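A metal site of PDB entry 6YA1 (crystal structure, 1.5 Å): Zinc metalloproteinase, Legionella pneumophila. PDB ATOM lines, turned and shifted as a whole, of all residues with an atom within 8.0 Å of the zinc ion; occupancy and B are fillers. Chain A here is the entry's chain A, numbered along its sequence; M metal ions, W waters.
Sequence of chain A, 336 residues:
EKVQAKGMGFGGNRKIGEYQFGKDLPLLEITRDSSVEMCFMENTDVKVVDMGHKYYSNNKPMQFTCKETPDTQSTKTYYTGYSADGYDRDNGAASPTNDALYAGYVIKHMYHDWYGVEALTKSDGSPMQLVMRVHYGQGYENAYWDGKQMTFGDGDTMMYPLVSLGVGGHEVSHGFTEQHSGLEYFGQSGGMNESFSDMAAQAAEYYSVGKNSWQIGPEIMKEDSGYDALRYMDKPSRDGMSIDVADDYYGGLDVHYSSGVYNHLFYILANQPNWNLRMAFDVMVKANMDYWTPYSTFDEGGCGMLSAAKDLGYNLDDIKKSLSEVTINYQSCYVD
Of the 21 residues printed, 4 come within 4 Å of the zinc ion. The nearest printed residue that does not touch the zinc ion is Arg 89 (5.7 Å).
The zinc ion is bound by OD2 of Asp 90, at 1.9 Å. OD2 of Asp 154 is bound to the zinc ion, at 1.9 Å. A ring nitrogen (NE2) of His 53 binds the zinc ion, at 2.1 Å. A ring nitrogen (ND1) of His 135 is bound to the zinc ion. Slightly farther from the zinc ion lies water W1 (2.7 Å).
The backbone carbonyl oxygen (O) of Asp 154 sits at hydrogen-bond distance from the side-chain amide nitrogen (ND2) of Asn 91. OD2 of Asp 88 is in hydrogen-bond range of NE2 of His 135 (2.6 Å).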
ATOM      1  N   ASP A  50     -21.448  -7.455   4.713  1.00  0.00           N
ATOM      2  CA  ASP A  50     -20.937  -6.503   5.692  1.00  0.00           C
ATOM      3  C   ASP A  50     -21.082  -7.116   7.079  1.00  0.00           C
ATOM      4  O   ASP A  50     -22.194  -7.171   7.648  1.00  0.00           O
ATOM      5  CB  ASP A  50     -21.654  -5.163   5.579  1.00  0.00           C
ATOM      6  CG  ASP A  50     -21.184  -4.149   6.597  1.00  0.00           C
ATOM      7  OD1 ASP A  50     -20.325  -4.474   7.464  1.00  0.00           O
ATOM      8  OD2 ASP A  50     -21.690  -3.002   6.524  1.00  0.00           O
ATOM      9  N   MET A  51     -19.964  -7.585   7.624  1.00  0.00           N
ATOM     10  CA  MET A  51     -19.986  -8.232   8.935  1.00  0.00           C
ATOM     11  C   MET A  51     -20.259  -7.264  10.073  1.00  0.00           C
ATOM     12  O   MET A  51     -20.523  -7.733  11.184  1.00  0.00           O
ATOM     13  CB  MET A  51     -18.669  -8.974   9.179  1.00  0.00           C
ATOM     14  CG  MET A  51     -18.342 -10.090   8.179  1.00  0.00           C
ATOM     15  SD  MET A  51     -19.441 -11.484   8.249  1.00  0.00           S
ATOM     16  CE  MET A  51     -19.101 -12.132   9.909  1.00  0.00           C
ATOM     17  N   GLY A  52     -20.217  -5.957   9.846  1.00  0.00           N
ATOM     18  CA  GLY A  52     -20.515  -5.016  10.910  1.00  0.00           C
ATOM     19  C   GLY A  52     -19.617  -5.191  12.110  1.00  0.00           C
ATOM     20  O   GLY A  52     -20.047  -4.949  13.252  1.00  0.00           O
ATOM     21  N   HIS A  53     -18.371  -5.606  11.867  1.00  0.00           N
ATOM     22  CA  HIS A  53     -17.336  -5.754  12.878  1.00  0.00           C
ATOM     23  C   HIS A  53     -17.611  -6.868  13.862  1.00  0.00           C
ATOM     24  O   HIS A  53     -17.006  -6.899  14.939  1.00  0.00           O
ATOM     25  CB  HIS A  53     -17.061  -4.441  13.568  1.00  0.00           C
ATOM     26  CG  HIS A  53     -16.785  -3.377  12.588  1.00  0.00           C
ATOM     27  ND1 HIS A  53     -17.480  -2.181  12.558  1.00  0.00           N
ATOM     28  CD2 HIS A  53     -15.993  -3.385  11.511  1.00  0.00           C
ATOM     29  CE1 HIS A  53     -17.045  -1.458  11.542  1.00  0.00           C
ATOM     30  NE2 HIS A  53     -16.137  -2.167  10.897  1.00  0.00           N
ATOM     31  N   ASP A  88     -17.731   3.840   1.817  1.00  0.00           N
ATOM     32  CA  ASP A  88     -17.950   2.952   2.956  1.00  0.00           C
ATOM     33  C   ASP A  88     -16.629   2.999   3.712  1.00  0.00           C
ATOM     34  O   ASP A  88     -15.891   2.031   3.819  1.00  0.00           O
ATOM     35  CB  ASP A  88     -18.317   1.545   2.471  1.00  0.00           C
ATOM     36  CG  ASP A  88     -18.500   0.557   3.610  1.00  0.00           C
ATOM     37  OD1 ASP A  88     -18.914   0.957   4.715  1.00  0.00           O
ATOM     38  OD2 ASP A  88     -18.230  -0.640   3.396  1.00  0.00           O
ATOM     39  N   ARG A  89     -16.319   4.179   4.256  1.00  0.00           N
ATOM     40  CA  ARG A  89     -14.971   4.450   4.713  1.00  0.00           C
ATOM     41  C   ARG A  89     -14.619   3.613   5.941  1.00  0.00           C
ATOM     42  O   ARG A  89     -15.461   3.350   6.804  1.00  0.00           O
ATOM     43  CB  ARG A  89     -14.820   5.939   5.039  1.00  0.00           C
ATOM     44  CG  ARG A  89     -14.987   6.874   3.848  1.00  0.00           C
ATOM     45  CD  ARG A  89     -14.431   8.252   4.182  1.00  0.00           C
ATOM     46  NE  ARG A  89     -14.304   9.167   3.039  1.00  0.00           N
ATOM     47  CZ  ARG A  89     -13.263   9.198   2.220  1.00  0.00           C
ATOM     48  NH1 ARG A  89     -12.255   8.361   2.371  1.00  0.00           N
ATOM     49  NH2 ARG A  89     -13.226  10.085   1.228  1.00  0.00           N
ATOM     50  N   ASP A  90     -13.361   3.185   6.004  1.00  0.00           N
ATOM     51  CA  ASP A  90     -12.911   2.359   7.104  1.00  0.00           C
ATOM     52  C   ASP A  90     -11.398   2.339   7.165  1.00  0.00           C
ATOM     53  O   ASP A  90     -10.728   1.966   6.191  1.00  0.00           O
ATOM     54  CB  ASP A  90     -13.469   0.938   6.959  1.00  0.00           C
ATOM     55  CG  ASP A  90     -13.554   0.249   8.271  1.00  0.00           C
ATOM     56  OD1 ASP A  90     -12.454   0.053   8.835  1.00  0.00           O
ATOM     57  OD2 ASP A  90     -14.682  -0.055   8.750  1.00  0.00           O
ATOM     58  N   ASN A  91     -10.845   2.714   8.314  1.00  0.00           N
ATOM     59  CA  ASN A  91      -9.402   2.641   8.598  1.00  0.00           C
ATOM     60  C   ASN A  91      -8.547   3.046   7.401  1.00  0.00           C
ATOM     61  O   ASN A  91      -7.610   2.349   6.995  1.00  0.00           O
ATOM     62  CB  ASN A  91      -9.018   1.233   9.036  1.00  0.00           C
ATOM     63  CG  ASN A  91      -7.596   1.140   9.557  1.00  0.00           C
ATOM     64  OD1 ASN A  91      -7.035   2.114  10.083  1.00  0.00           O
ATOM     65  ND2 ASN A  91      -7.002  -0.052   9.430  1.00  0.00           N
ATOM     66  N   PRO A  96     -14.023  -0.641   1.523  1.00  0.00           N
ATOM     67  CA  PRO A  96     -13.589  -2.049   1.389  1.00  0.00           C
ATOM     68  C   PRO A  96     -14.661  -2.922   0.764  1.00  0.00           C
ATOM     69  O   PRO A  96     -14.322  -3.926   0.116  1.00  0.00           O
ATOM     70  CB  PRO A  96     -13.260  -2.467   2.823  1.00  0.00           C
ATOM     71  CG  PRO A  96     -13.010  -1.140   3.570  1.00  0.00           C
ATOM     72  CD  PRO A  96     -13.904  -0.124   2.906  1.00  0.00           C
ATOM     73  N   THR A  97     -15.945  -2.594   0.939  1.00  0.00           N
ATOM     74  CA  THR A  97     -16.982  -3.415   0.328  1.00  0.00           C
ATOM     75  C   THR A  97     -16.992  -3.269  -1.193  1.00  0.00           C
ATOM     76  O   THR A  97     -17.146  -4.269  -1.904  1.00  0.00           O
ATOM     77  CB  THR A  97     -18.340  -3.082   0.919  1.00  0.00           C
ATOM     78  OG1 THR A  97     -18.525  -1.667   0.952  1.00  0.00           O
ATOM     79  CG2 THR A  97     -18.442  -3.631   2.340  1.00  0.00           C
ATOM     80  N   VAL A 134     -16.626  -8.861   4.609  1.00  0.00           N
ATOM     81  CA  VAL A 134     -15.850  -7.653   4.788  1.00  0.00           C
ATOM     82  C   VAL A 134     -16.246  -7.010   6.134  1.00  0.00           C
ATOM     83  O   VAL A 134     -17.283  -7.336   6.694  1.00  0.00           O
ATOM     84  CB  VAL A 134     -16.074  -6.689   3.598  1.00  0.00           C
ATOM     85  CG1 VAL A 134     -15.195  -5.465   3.706  1.00  0.00           C
ATOM     86  CG2 VAL A 134     -15.781  -7.423   2.274  1.00  0.00           C
ATOM     87  N   HIS A 135     -15.409  -6.104   6.628  1.00  0.00           N
ATOM     88  CA  HIS A 135     -15.622  -5.499   7.952  1.00  0.00           C
ATOM     89  C   HIS A 135     -15.644  -6.568   9.038  1.00  0.00           C
ATOM     90  O   HIS A 135     -16.393  -6.469  10.013  1.00  0.00           O
ATOM     91  CB  HIS A 135     -16.922  -4.670   8.012  1.00  0.00           C
ATOM     92  CG  HIS A 135     -16.959  -3.522   7.043  1.00  0.00           C
ATOM     93  ND1 HIS A 135     -16.223  -2.374   7.230  1.00  0.00           N
ATOM     94  CD2 HIS A 135     -17.676  -3.317   5.908  1.00  0.00           C
ATOM     95  CE1 HIS A 135     -16.426  -1.533   6.227  1.00  0.00           C
ATOM     96  NE2 HIS A 135     -17.323  -2.067   5.426  1.00  0.00           N
ATOM     97  N   TYR A 136     -14.842  -7.610   8.871  1.00  0.00           N
ATOM     98  CA  TYR A 136     -14.850  -8.710   9.824  1.00  0.00           C
ATOM     99  C   TYR A 136     -14.113  -8.339  11.098  1.00  0.00           C
ATOM    100  O   TYR A 136     -12.961  -7.926  11.049  1.00  0.00           O
ATOM    101  CB  TYR A 136     -14.145  -9.904   9.206  1.00  0.00           C
ATOM    102  CG  TYR A 136     -14.021 -11.130  10.071  1.00  0.00           C
ATOM    103  CD1 TYR A 136     -15.088 -12.014  10.228  1.00  0.00           C
ATOM    104  CD2 TYR A 136     -12.824 -11.420  10.687  1.00  0.00           C
ATOM    105  CE1 TYR A 136     -14.930 -13.158  10.983  1.00  0.00           C
ATOM    106  CE2 TYR A 136     -12.666 -12.544  11.440  1.00  0.00           C
ATOM    107  CZ  TYR A 136     -13.712 -13.408  11.587  1.00  0.00           C
ATOM    108  OH  TYR A 136     -13.519 -14.542  12.346  1.00  0.00           O
ATOM    109  N   GLY A 137     -14.784  -8.474  12.238  1.00  0.00           N
ATOM    110  CA  GLY A 137     -14.129  -8.256  13.516  1.00  0.00           C
ATOM    111  C   GLY A 137     -13.804  -6.787  13.799  1.00  0.00           C
ATOM    112  O   GLY A 137     -14.197  -5.876  13.079  1.00  0.00           O
ATOM    113  N   GLN A 138     -13.101  -6.582  14.919  1.00  0.00           N
ATOM    114  CA  GLN A 138     -12.679  -5.259  15.351  1.00  0.00           C
ATOM    115  C   GLN A 138     -11.161  -5.211  15.277  1.00  0.00           C
ATOM    116  O   GLN A 138     -10.473  -5.902  16.031  1.00  0.00           O
ATOM    117  CB  GLN A 138     -13.144  -4.953  16.766  1.00  0.00           C
ATOM    118  CG  GLN A 138     -14.649  -5.012  16.932  1.00  0.00           C
ATOM    119  CD  GLN A 138     -15.090  -5.043  18.391  1.00  0.00           C
ATOM    120  OE1 GLN A 138     -15.138  -4.012  19.055  1.00  0.00           O
ATOM    121  NE2 GLN A 138     -15.408  -6.232  18.887  1.00  0.00           N
ATOM    122  N   GLY A 139     -10.628  -4.385  14.382  1.00  0.00           N
ATOM    123  CA  GLY A 139      -9.197  -4.239  14.304  1.00  0.00           C
ATOM    124  C   GLY A 139      -8.492  -5.504  13.893  1.00  0.00           C
ATOM    125  O   GLY A 139      -7.363  -5.762  14.325  1.00  0.00           O
ATOM    126  N   PHE A 152     -12.204 -10.958   5.430  1.00  0.00           N
ATOM    127  CA  PHE A 152     -11.234  -9.888   5.362  1.00  0.00           C
ATOM    128  C   PHE A 152     -11.422  -8.897   6.507  1.00  0.00           C
ATOM    129  O   PHE A 152     -12.482  -8.258   6.619  1.00  0.00           O
ATOM    130  CB  PHE A 152     -11.315  -9.145   4.019  1.00  0.00           C
ATOM    131  CG  PHE A 152     -11.303 -10.036   2.804  1.00  0.00           C
ATOM    132  CD1 PHE A 152     -12.466 -10.570   2.289  1.00  0.00           C
ATOM    133  CD2 PHE A 152     -10.113 -10.329   2.141  1.00  0.00           C
ATOM    134  CE1 PHE A 152     -12.457 -11.403   1.161  1.00  0.00           C
ATOM    135  CE2 PHE A 152     -10.104 -11.152   1.013  1.00  0.00           C
ATOM    136  CZ  PHE A 152     -11.259 -11.674   0.517  1.00  0.00           C
ATOM    137  N   GLY A 153     -10.366  -8.695   7.272  1.00  0.00           N
ATOM    138  CA  GLY A 153     -10.374  -7.707   8.336  1.00  0.00           C
ATOM    139  C   GLY A 153     -10.209  -6.291   7.836  1.00  0.00           C
ATOM    140  O   GLY A 153      -9.888  -6.035   6.684  1.00  0.00           O
ATOM    141  N   ASP A 154     -10.483  -5.334   8.733  1.00  0.00           N
ATOM    142  CA  ASP A 154     -10.258  -3.933   8.394  1.00  0.00           C
ATOM    143  C   ASP A 154      -8.843  -3.480   8.724  1.00  0.00           C
ATOM    144  O   ASP A 154      -8.498  -2.334   8.430  1.00  0.00           O
ATOM    145  CB  ASP A 154     -11.234  -3.026   9.139  1.00  0.00           C
ATOM    146  CG  ASP A 154     -12.620  -3.085   8.594  1.00  0.00           C
ATOM    147  OD1 ASP A 154     -12.790  -3.297   7.386  1.00  0.00           O
ATOM    148  OD2 ASP A 154     -13.560  -2.896   9.380  1.00  0.00           O
ATOM    149  N   GLY A 155      -8.035  -4.325   9.300  1.00  0.00           N
ATOM    150  CA  GLY A 155      -6.725  -3.904   9.753  1.00  0.00           C
ATOM    151  C   GLY A 155      -6.783  -3.080  11.012  1.00  0.00           C
ATOM    152  O   GLY A 155      -7.835  -2.841  11.601  1.00  0.00           O
ATOM    153  N   PRO A 161      -7.546  -1.912   5.469  1.00  0.00           N
ATOM    154  CA  PRO A 161      -8.453  -3.046   5.262  1.00  0.00           C
ATOM    155  C   PRO A 161      -7.870  -3.989   4.210  1.00  0.00           C
ATOM    156  O   PRO A 161      -7.396  -3.559   3.169  1.00  0.00           O
ATOM    157  CB  PRO A 161      -9.753  -2.372   4.810  1.00  0.00           C
ATOM    158  CG  PRO A 161      -9.741  -1.025   5.612  1.00  0.00           C
ATOM    159  CD  PRO A 161      -8.270  -0.613   5.580  1.00  0.00           C
HETATM  160 ZN    ZN M   1     -15.178  -1.889   9.037  1.00  0.00          ZN
HETATM  161  O   HOH W   1     -13.345  -1.012  10.755  1.00  0.00           O
